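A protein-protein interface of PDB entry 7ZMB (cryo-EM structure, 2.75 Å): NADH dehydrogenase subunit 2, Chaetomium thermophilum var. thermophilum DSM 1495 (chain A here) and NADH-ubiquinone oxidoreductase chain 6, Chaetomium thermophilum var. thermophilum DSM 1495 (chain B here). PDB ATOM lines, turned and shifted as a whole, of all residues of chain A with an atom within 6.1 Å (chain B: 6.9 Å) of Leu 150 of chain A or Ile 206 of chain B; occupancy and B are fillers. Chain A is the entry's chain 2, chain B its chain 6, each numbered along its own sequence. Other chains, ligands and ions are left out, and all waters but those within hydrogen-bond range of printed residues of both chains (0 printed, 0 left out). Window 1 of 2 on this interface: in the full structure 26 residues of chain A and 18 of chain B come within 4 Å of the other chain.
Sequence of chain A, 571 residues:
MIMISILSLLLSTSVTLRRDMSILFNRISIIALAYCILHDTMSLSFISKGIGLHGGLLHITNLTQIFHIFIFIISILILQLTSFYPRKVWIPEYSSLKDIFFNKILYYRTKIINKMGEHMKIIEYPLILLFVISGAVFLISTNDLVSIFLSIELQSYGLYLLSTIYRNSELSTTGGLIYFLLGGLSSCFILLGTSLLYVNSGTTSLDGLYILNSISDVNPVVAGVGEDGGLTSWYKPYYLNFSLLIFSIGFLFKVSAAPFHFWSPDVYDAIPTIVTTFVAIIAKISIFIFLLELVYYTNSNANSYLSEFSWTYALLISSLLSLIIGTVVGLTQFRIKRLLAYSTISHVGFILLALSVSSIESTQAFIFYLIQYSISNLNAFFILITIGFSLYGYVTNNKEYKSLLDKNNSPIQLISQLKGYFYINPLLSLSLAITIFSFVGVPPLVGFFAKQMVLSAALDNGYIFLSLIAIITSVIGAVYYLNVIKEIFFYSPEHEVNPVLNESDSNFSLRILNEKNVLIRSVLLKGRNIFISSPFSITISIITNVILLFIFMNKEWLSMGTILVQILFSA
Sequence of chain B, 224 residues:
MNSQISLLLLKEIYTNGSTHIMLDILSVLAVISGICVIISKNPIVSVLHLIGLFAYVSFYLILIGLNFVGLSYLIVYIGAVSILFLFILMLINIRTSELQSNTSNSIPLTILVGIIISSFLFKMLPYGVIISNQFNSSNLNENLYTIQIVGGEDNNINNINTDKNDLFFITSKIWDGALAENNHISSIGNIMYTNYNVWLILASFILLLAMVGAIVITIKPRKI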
ATOM      1  N   PHE A 131      -0.401 -27.358   5.266  1.00  0.00           N
ATOM      2  CA  PHE A 131       0.744 -27.015   4.386  1.00  0.00           C
ATOM      3  C   PHE A 131       0.254 -26.654   2.977  1.00  0.00           C
ATOM      4  O   PHE A 131       0.841 -25.762   2.360  1.00  0.00           O
ATOM      5  CB  PHE A 131       1.716 -28.194   4.306  1.00  0.00           C
ATOM      6  CG  PHE A 131       2.781 -28.274   5.365  1.00  0.00           C
ATOM      7  CD1 PHE A 131       3.858 -27.403   5.358  1.00  0.00           C
ATOM      8  CD2 PHE A 131       2.742 -29.266   6.330  1.00  0.00           C
ATOM      9  CE1 PHE A 131       4.849 -27.501   6.320  1.00  0.00           C
ATOM     10  CE2 PHE A 131       3.734 -29.360   7.291  1.00  0.00           C
ATOM     11  CZ  PHE A 131       4.785 -28.478   7.283  1.00  0.00           C
ATOM     12  N   LEU A 145       9.312 -13.814  -9.064  1.00  0.00           N
ATOM     13  CA  LEU A 145       9.380 -15.088  -9.818  1.00  0.00           C
ATOM     14  C   LEU A 145       9.788 -16.226  -8.879  1.00  0.00           C
ATOM     15  O   LEU A 145       9.165 -17.286  -8.965  1.00  0.00           O
ATOM     16  CB  LEU A 145      10.354 -14.928 -10.986  1.00  0.00           C
ATOM     17  CG  LEU A 145       9.857 -14.063 -12.141  1.00  0.00           C
ATOM     18  CD1 LEU A 145      10.973 -13.812 -13.139  1.00  0.00           C
ATOM     19  CD2 LEU A 145       8.659 -14.707 -12.821  1.00  0.00           C
ATOM     20  N   VAL A 146      10.771 -15.999  -8.006  1.00  0.00           N
ATOM     21  CA  VAL A 146      11.232 -17.059  -7.115  1.00  0.00           C
ATOM     22  C   VAL A 146      10.146 -17.423  -6.110  1.00  0.00           C
ATOM     23  O   VAL A 146       9.971 -18.596  -5.763  1.00  0.00           O
ATOM     24  CB  VAL A 146      12.545 -16.634  -6.424  1.00  0.00           C
ATOM     25  CG1 VAL A 146      13.086 -17.731  -5.516  1.00  0.00           C
ATOM     26  CG2 VAL A 146      13.587 -16.231  -7.459  1.00  0.00           C
ATOM     27  N   SER A 147       9.386 -16.430  -5.644  1.00  0.00           N
ATOM     28  CA  SER A 147       8.287 -16.703  -4.722  1.00  0.00           C
ATOM     29  C   SER A 147       7.216 -17.576  -5.363  1.00  0.00           C
ATOM     30  O   SER A 147       6.606 -18.413  -4.690  1.00  0.00           O
ATOM     31  CB  SER A 147       7.675 -15.397  -4.230  1.00  0.00           C
ATOM     32  OG  SER A 147       8.574 -14.704  -3.398  1.00  0.00           O
ATOM     33  N   ILE A 148       6.958 -17.384  -6.656  1.00  0.00           N
ATOM     34  CA  ILE A 148       5.948 -18.185  -7.344  1.00  0.00           C
ATOM     35  C   ILE A 148       6.345 -19.652  -7.337  1.00  0.00           C
ATOM     36  O   ILE A 148       5.534 -20.534  -7.037  1.00  0.00           O
ATOM     37  CB  ILE A 148       5.739 -17.669  -8.780  1.00  0.00           C
ATOM     38  CG1 ILE A 148       4.906 -16.392  -8.781  1.00  0.00           C
ATOM     39  CG2 ILE A 148       5.075 -18.721  -9.647  1.00  0.00           C
ATOM     40  CD1 ILE A 148       5.221 -15.465  -9.924  1.00  0.00           C
ATOM     41  N   PHE A 149       7.603 -19.934  -7.669  1.00  0.00           N
ATOM     42  CA  PHE A 149       8.037 -21.317  -7.814  1.00  0.00           C
ATOM     43  C   PHE A 149       7.992 -22.058  -6.482  1.00  0.00           C
ATOM     44  O   PHE A 149       7.549 -23.209  -6.422  1.00  0.00           O
ATOM     45  CB  PHE A 149       9.439 -21.351  -8.416  1.00  0.00           C
ATOM     46  CG  PHE A 149      10.012 -22.723  -8.537  1.00  0.00           C
ATOM     47  CD1 PHE A 149       9.505 -23.621  -9.460  1.00  0.00           C
ATOM     48  CD2 PHE A 149      11.069 -23.111  -7.753  1.00  0.00           C
ATOM     49  CE1 PHE A 149      10.038 -24.883  -9.583  1.00  0.00           C
ATOM     50  CE2 PHE A 149      11.601 -24.365  -7.880  1.00  0.00           C
ATOM     51  CZ  PHE A 149      11.085 -25.253  -8.792  1.00  0.00           C
ATOM     52  N   LEU A 150       8.447 -21.418  -5.402  1.00  0.00           N
ATOM     53  CA  LEU A 150       8.431 -22.075  -4.099  1.00  0.00           C
ATOM     54  C   LEU A 150       7.006 -22.295  -3.611  1.00  0.00           C
ATOM     55  O   LEU A 150       6.712 -23.305  -2.964  1.00  0.00           O
ATOM     56  CB  LEU A 150       9.224 -21.257  -3.081  1.00  0.00           C
ATOM     57  CG  LEU A 150      10.699 -20.983  -3.369  1.00  0.00           C
ATOM     58  CD1 LEU A 150      11.123 -19.643  -2.806  1.00  0.00           C
ATOM     59  CD2 LEU A 150      11.586 -22.080  -2.835  1.00  0.00           C
ATOM     60  N   SER A 151       6.106 -21.361  -3.912  1.00  0.00           N
ATOM     61  CA  SER A 151       4.736 -21.470  -3.428  1.00  0.00           C
ATOM     62  C   SER A 151       3.945 -22.528  -4.185  1.00  0.00           C
ATOM     63  O   SER A 151       3.155 -23.258  -3.580  1.00  0.00           O
ATOM     64  CB  SER A 151       4.042 -20.115  -3.515  1.00  0.00           C
ATOM     65  OG  SER A 151       4.532 -19.241  -2.521  1.00  0.00           O
ATOM     66  N   ILE A 152       4.138 -22.632  -5.499  1.00  0.00           N
ATOM     67  CA  ILE A 152       3.426 -23.670  -6.233  1.00  0.00           C
ATOM     68  C   ILE A 152       3.928 -25.053  -5.834  1.00  0.00           C
ATOM     69  O   ILE A 152       3.156 -26.015  -5.824  1.00  0.00           O
ATOM     70  CB  ILE A 152       3.507 -23.426  -7.754  1.00  0.00           C
ATOM     71  CG1 ILE A 152       2.392 -24.181  -8.480  1.00  0.00           C
ATOM     72  CG2 ILE A 152       4.862 -23.800  -8.317  1.00  0.00           C
ATOM     73  CD1 ILE A 152       1.009 -23.794  -8.043  1.00  0.00           C
ATOM     74  N   GLU A 153       5.205 -25.128  -5.458  1.00  0.00           N
ATOM     75  CA  GLU A 153       5.779 -26.422  -5.021  1.00  0.00           C
ATOM     76  C   GLU A 153       5.180 -26.779  -3.667  1.00  0.00           C
ATOM     77  O   GLU A 153       4.733 -27.915  -3.512  1.00  0.00           O
ATOM     78  CB  GLU A 153       7.300 -26.353  -4.924  1.00  0.00           C
ATOM     79  CG  GLU A 153       8.016 -26.138  -6.245  1.00  0.00           C
ATOM     80  CD  GLU A 153       7.767 -27.157  -7.341  1.00  0.00           C
ATOM     81  OE1 GLU A 153       8.688 -27.942  -7.626  1.00  0.00           O
ATOM     82  OE2 GLU A 153       6.669 -27.142  -7.926  1.00  0.00           O
ATOM     83  N   LEU A 154       5.180 -25.835  -2.729  1.00  0.00           N
ATOM     84  CA  LEU A 154       4.623 -26.102  -1.408  1.00  0.00           C
ATOM     85  C   LEU A 154       3.159 -26.504  -1.496  1.00  0.00           C
ATOM     86  O   LEU A 154       2.683 -27.291  -0.673  1.00  0.00           O
ATOM     87  CB  LEU A 154       4.791 -24.886  -0.501  1.00  0.00           C
ATOM     88  CG  LEU A 154       4.293 -25.029   0.941  1.00  0.00           C
ATOM     89  CD1 LEU A 154       4.888 -26.248   1.620  1.00  0.00           C
ATOM     90  CD2 LEU A 154       4.582 -23.784   1.740  1.00  0.00           C
ATOM     91  N   GLN A 155       2.427 -25.975  -2.477  1.00  0.00           N
ATOM     92  CA  GLN A 155       1.062 -26.432  -2.713  1.00  0.00           C
ATOM     93  C   GLN A 155       1.039 -27.807  -3.370  1.00  0.00           C
ATOM     94  O   GLN A 155       0.246 -28.672  -2.987  1.00  0.00           O
ATOM     95  CB  GLN A 155       0.314 -25.410  -3.567  1.00  0.00           C
ATOM     96  CG  GLN A 155      -1.185 -25.639  -3.669  1.00  0.00           C
ATOM     97  CD  GLN A 155      -1.791 -25.013  -4.910  1.00  0.00           C
ATOM     98  OE1 GLN A 155      -1.987 -23.806  -4.978  1.00  0.00           O
ATOM     99  NE2 GLN A 155      -2.069 -25.832  -5.908  1.00  0.00           N
ATOM    100  N   TYR A 157       3.422 -30.324  -3.632  1.00  0.00           N
ATOM    101  CA  TYR A 157       4.008 -31.449  -2.920  1.00  0.00           C
ATOM    102  C   TYR A 157       3.047 -31.982  -1.870  1.00  0.00           C
ATOM    103  O   TYR A 157       2.933 -33.197  -1.680  1.00  0.00           O
ATOM    104  CB  TYR A 157       5.321 -31.020  -2.273  1.00  0.00           C
ATOM    105  CG  TYR A 157       6.420 -30.817  -3.274  1.00  0.00           C
ATOM    106  CD1 TYR A 157       6.382 -31.441  -4.501  1.00  0.00           C
ATOM    107  CD2 TYR A 157       7.461 -29.940  -3.017  1.00  0.00           C
ATOM    108  CE1 TYR A 157       7.358 -31.233  -5.432  1.00  0.00           C
ATOM    109  CE2 TYR A 157       8.452 -29.730  -3.940  1.00  0.00           C
ATOM    110  CZ  TYR A 157       8.390 -30.377  -5.147  1.00  0.00           C
ATOM    111  OH  TYR A 157       9.366 -30.169  -6.089  1.00  0.00           O
ATOM    112  N   VAL B 198      12.301 -14.256   3.101  1.00  0.00           N
ATOM    113  CA  VAL B 198      10.995 -14.908   2.803  1.00  0.00           C
ATOM    114  C   VAL B 198      11.257 -16.210   2.046  1.00  0.00           C
ATOM    115  O   VAL B 198      10.629 -17.216   2.366  1.00  0.00           O
ATOM    116  CB  VAL B 198      10.054 -13.952   2.040  1.00  0.00           C
ATOM    117  CG1 VAL B 198       9.213 -14.646   0.979  1.00  0.00           C
ATOM    118  CG2 VAL B 198       9.180 -13.142   2.983  1.00  0.00           C
ATOM    119  N   TRP B 199      12.209 -16.203   1.129  1.00  0.00           N
ATOM    120  CA  TRP B 199      12.537 -17.412   0.341  1.00  0.00           C
ATOM    121  C   TRP B 199      13.107 -18.460   1.279  1.00  0.00           C
ATOM    122  O   TRP B 199      12.777 -19.621   1.091  1.00  0.00           O
ATOM    123  CB  TRP B 199      13.512 -17.107  -0.800  1.00  0.00           C
ATOM    124  CG  TRP B 199      13.003 -16.151  -1.831  1.00  0.00           C
ATOM    125  CD1 TRP B 199      11.706 -15.805  -2.079  1.00  0.00           C
ATOM    126  CD2 TRP B 199      13.799 -15.431  -2.786  1.00  0.00           C
ATOM    127  NE1 TRP B 199      11.644 -14.913  -3.114  1.00  0.00           N
ATOM    128  CE2 TRP B 199      12.911 -14.665  -3.569  1.00  0.00           C
ATOM    129  CE3 TRP B 199      15.171 -15.358  -3.050  1.00  0.00           C
ATOM    130  CZ2 TRP B 199      13.354 -13.836  -4.597  1.00  0.00           C
ATOM    131  CZ3 TRP B 199      15.606 -14.541  -4.067  1.00  0.00           C
ATOM    132  CH2 TRP B 199      14.708 -13.792  -4.827  1.00  0.00           C
ATOM    133  N   LEU B 200      13.917 -18.045   2.254  1.00  0.00           N
ATOM    134  CA  LEU B 200      14.427 -18.992   3.237  1.00  0.00           C
ATOM    135  C   LEU B 200      13.303 -19.574   4.085  1.00  0.00           C
ATOM    136  O   LEU B 200      13.300 -20.772   4.382  1.00  0.00           O
ATOM    137  CB  LEU B 200      15.467 -18.310   4.116  1.00  0.00           C
ATOM    138  CG  LEU B 200      16.173 -19.159   5.167  1.00  0.00           C
ATOM    139  CD1 LEU B 200      17.124 -20.115   4.518  1.00  0.00           C
ATOM    140  CD2 LEU B 200      16.908 -18.261   6.136  1.00  0.00           C
ATOM    141  N   ILE B 201      12.341 -18.744   4.485  1.00  0.00           N
ATOM    142  CA  ILE B 201      11.252 -19.227   5.326  1.00  0.00           C
ATOM    143  C   ILE B 201      10.357 -20.184   4.547  1.00  0.00           C
ATOM    144  O   ILE B 201       9.999 -21.258   5.040  1.00  0.00           O
ATOM    145  CB  ILE B 201      10.469 -18.043   5.921  1.00  0.00           C
ATOM    146  CG1 ILE B 201      11.377 -17.218   6.821  1.00  0.00           C
ATOM    147  CG2 ILE B 201       9.338 -18.535   6.760  1.00  0.00           C
ATOM    148  CD1 ILE B 201      10.856 -15.867   7.157  1.00  0.00           C
ATOM    149  N   LEU B 202      10.005 -19.826   3.310  1.00  0.00           N
ATOM    150  CA  LEU B 202       9.267 -20.750   2.452  1.00  0.00           C
ATOM    151  C   LEU B 202      10.063 -22.013   2.166  1.00  0.00           C
ATOM    152  O   LEU B 202       9.515 -23.119   2.206  1.00  0.00           O
ATOM    153  CB  LEU B 202       8.868 -20.069   1.143  1.00  0.00           C
ATOM    154  CG  LEU B 202       7.612 -19.208   1.043  1.00  0.00           C
ATOM    155  CD1 LEU B 202       6.392 -20.067   1.274  1.00  0.00           C
ATOM    156  CD2 LEU B 202       7.622 -18.061   2.035  1.00  0.00           C
ATOM    157  N   ALA B 203      11.346 -21.868   1.845  1.00  0.00           N
ATOM    158  CA  ALA B 203      12.221 -23.041   1.603  1.00  0.00           C
ATOM    159  C   ALA B 203      12.101 -24.010   2.776  1.00  0.00           C
ATOM    160  O   ALA B 203      11.967 -25.221   2.541  1.00  0.00           O
ATOM    161  CB  ALA B 203      13.634 -22.623   1.334  1.00  0.00           C
ATOM    162  N   SER B 204      12.213 -23.472   3.990  1.00  0.00           N
ATOM    163  CA  SER B 204      12.179 -24.283   5.226  1.00  0.00           C
ATOM    164  C   SER B 204      10.861 -25.044   5.344  1.00  0.00           C
ATOM    165  O   SER B 204      10.894 -26.191   5.808  1.00  0.00           O
ATOM    166  CB  SER B 204      12.402 -23.389   6.414  1.00  0.00           C
ATOM    167  OG  SER B 204      11.208 -22.733   6.799  1.00  0.00           O
ATOM    168  N   PHE B 205       9.747 -24.414   4.970  1.00  0.00           N
ATOM    169  CA  PHE B 205       8.425 -25.087   5.009  1.00  0.00           C
ATOM    170  C   PHE B 205       8.377 -26.256   4.015  1.00  0.00           C
ATOM    171  O   PHE B 205       7.782 -27.291   4.347  1.00  0.00           O
ATOM    172  CB  PHE B 205       7.279 -24.069   5.001  1.00  0.00           C
ATOM    173  CG  PHE B 205       6.856 -23.652   6.387  1.00  0.00           C
ATOM    174  CD1 PHE B 205       7.680 -22.866   7.174  1.00  0.00           C
ATOM    175  CD2 PHE B 205       5.652 -24.079   6.921  1.00  0.00           C
ATOM    176  CE1 PHE B 205       7.303 -22.504   8.458  1.00  0.00           C
ATOM    177  CE2 PHE B 205       5.274 -23.713   8.203  1.00  0.00           C
ATOM    178  CZ  PHE B 205       6.098 -22.924   8.968  1.00  0.00           C
ATOM    179  N   ILE B 206       8.966 -26.094   2.832  1.00  0.00           N
ATOM    180  CA  ILE B 206       8.993 -27.194   1.819  1.00  0.00           C
ATOM    181  C   ILE B 206       9.798 -28.364   2.392  1.00  0.00           C
ATOM    182  O   ILE B 206       9.321 -29.506   2.291  1.00  0.00           O
ATOM    183  CB  ILE B 206       9.536 -26.713   0.455  1.00  0.00           C
ATOM    184  CG1 ILE B 206       8.755 -25.502  -0.059  1.00  0.00           C
ATOM    185  CG2 ILE B 206       9.565 -27.841  -0.561  1.00  0.00           C
ATOM    186  CD1 ILE B 206       9.445 -24.757  -1.173  1.00  0.00           C
ATOM    187  N   LEU B 207      10.940 -28.070   3.014  1.00  0.00           N
ATOM    188  CA  LEU B 207      11.791 -29.125   3.621  1.00  0.00           C
ATOM    189  C   LEU B 207      11.041 -29.808   4.764  1.00  0.00           C
ATOM    190  O   LEU B 207      11.127 -31.035   4.855  1.00  0.00           O
ATOM    191  CB  LEU B 207      13.066 -28.467   4.137  1.00  0.00           C
ATOM    192  CG  LEU B 207      14.038 -27.982   3.073  1.00  0.00           C
ATOM    193  CD1 LEU B 207      14.794 -26.777   3.589  1.00  0.00           C
ATOM    194  CD2 LEU B 207      14.986 -29.096   2.663  1.00  0.00           C
ATOM    195  N   LEU B 208      10.321 -29.038   5.575  1.00  0.00           N
ATOM    196  CA  LEU B 208       9.550 -29.595   6.708  1.00  0.00           C
ATOM    197  C   LEU B 208       8.470 -30.544   6.189  1.00  0.00           C
ATOM    198  O   LEU B 208       8.324 -31.635   6.756  1.00  0.00           O
ATOM    199  CB  LEU B 208       8.910 -28.423   7.456  1.00  0.00           C
ATOM    200  CG  LEU B 208       8.326 -28.742   8.825  1.00  0.00           C
ATOM    201  CD1 LEU B 208       9.418 -29.256   9.737  1.00  0.00           C
ATOM    202  CD2 LEU B 208       7.672 -27.507   9.419  1.00  0.00           C
ATOM    203  N   LEU B 209       7.748 -30.140   5.149  1.00  0.00           N
ATOM    204  CA  LEU B 209       6.684 -30.996   4.585  1.00  0.00           C
ATOM    205  C   LEU B 209       7.317 -32.273   4.032  1.00  0.00           C
ATOM    206  O   LEU B 209       6.769 -33.351   4.295  1.00  0.00           O
ATOM    207  CB  LEU B 209       5.923 -30.194   3.526  1.00  0.00           C
ATOM    208  CG  LEU B 209       5.046 -30.974   2.551  1.00  0.00           C
ATOM    209  CD1 LEU B 209       3.745 -31.391   3.213  1.00  0.00           C
ATOM    210  CD2 LEU B 209       4.764 -30.133   1.319  1.00  0.00           C
ATOM    211  N   ALA B 210       8.454 -32.162   3.349  1.00  0.00           N
ATOM    212  CA  ALA B 210       9.159 -33.363   2.846  1.00  0.00           C
ATOM    213  C   ALA B 210       9.636 -34.253   4.002  1.00  0.00           C
ATOM    214  O   ALA B 210       9.492 -35.471   3.886  1.00  0.00           O
ATOM    215  CB  ALA B 210      10.282 -32.955   1.941  1.00  0.00           C
ATOM    216  N   MET B 211      10.165 -33.670   5.078  1.00  0.00           N
ATOM    217  CA  MET B 211      10.620 -34.439   6.269  1.00  0.00           C
ATOM    218  C   MET B 211       9.428 -35.142   6.930  1.00  0.00           C
ATOM    219  O   MET B 211       9.598 -36.277   7.375  1.00  0.00           O
ATOM    220  CB  MET B 211      11.322 -33.532   7.287  1.00  0.00           C
ATOM    221  CG  MET B 211      12.635 -32.960   6.809  1.00  0.00           C
ATOM    222  SD  MET B 211      13.368 -31.815   8.002  1.00  0.00           S
ATOM    223  CE  MET B 211      13.919 -32.959   9.266  1.00  0.00           C
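NE1 of Trp 199 of chain B sits at hydrogen-bond distance from OG of Ser 147 of chain A, 3.1 Å away.
The side-chain hydroxyl (OG) of Ser 151 of chain A sits at hydrogen-bond distance from the backbone carbonyl oxygen (O) of Ser 147 of chain A, 3.1 Å away.
OE1 of Glu 153 of chain A sits at hydrogen-bond distance from OH of Tyr 157 of chain A (2.8 Å).
Phe 131 of chain A touches Phe 205 of chain B (CE1 to O, 3.5 Å).
CD2 of Leu 208 of chain B touches CZ of Phe 131 of chain A, at 3.7 Å.
CD2 of Phe 131 of chain A touches CD1 of Leu 209 of chain B, at 3.9 Å.
Val 146 of chain A touches Trp 199 of chain B (CB to CZ2, 3.4 Å).
Trp 199 of chain B touches Leu 150 of chain A (CD1 to CD1, 3.9 Å).
Leu 150 of chain A touches Ile 206 of chain B (O to CD1, 3.6 Å).
CD1 of Leu 154 of chain A touches CD2 of Leu 209 of chain B (3.9 Å).
Ile 206 of chain B touches Tyr 157 of chain A.
Leu 209 of chain B touches Tyr 157 of chain A.
Leu 150 of chain A touches just these residues of chain B: Trp 199 (3.9 Å) and Ile 206 (3.6 Å).
Ile 206 of chain B touches just these residues of chain A: Leu 150 (3.6 Å) and Tyr 157 (3.9 Å).
Of the printed residues of chain B, Val 146 of chain A touches Trp 199 (3.4 Å).
Printed residues of chain B within 4 Å of Tyr 157 of chain A: Ile 206 (3.9 Å) and Leu 209 (3.7 Å).
Printed residues of chain A within 4 Å of Phe 205 of chain B: Phe 131 (3.5 Å).
Printed residues of chain B within 4 Å of Ser 147 of chain A: Trp 199 (3.1 Å).
Of the printed residues of chain A, Trp 199 of chain B touches Val 146, Ser 147 and Leu 150.
Ala 203 of chain B touches none of the printed residues of chain A.
Met 211 of chain B touches none of the printed residues of chain A.
The nearest residue of chain A that does not touch Ile 206 of chain B is Leu 154 of chain A (4.04 Å).
Of the 13 printed residues of chain A, 6 touch a printed residue of chain B.
Hydrophobic or aromatic side chains of chain A that line the printed part of chain B: Phe 131, Val 146, Leu 150, Leu 154 and Tyr 157.
Among the printed residues, 10 pairs touch across the chains.
Among the printed residues, no Asp or Glu carboxylate lies within 4 Å of a Lys or Arg side-chain nitrogen of the other chain.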
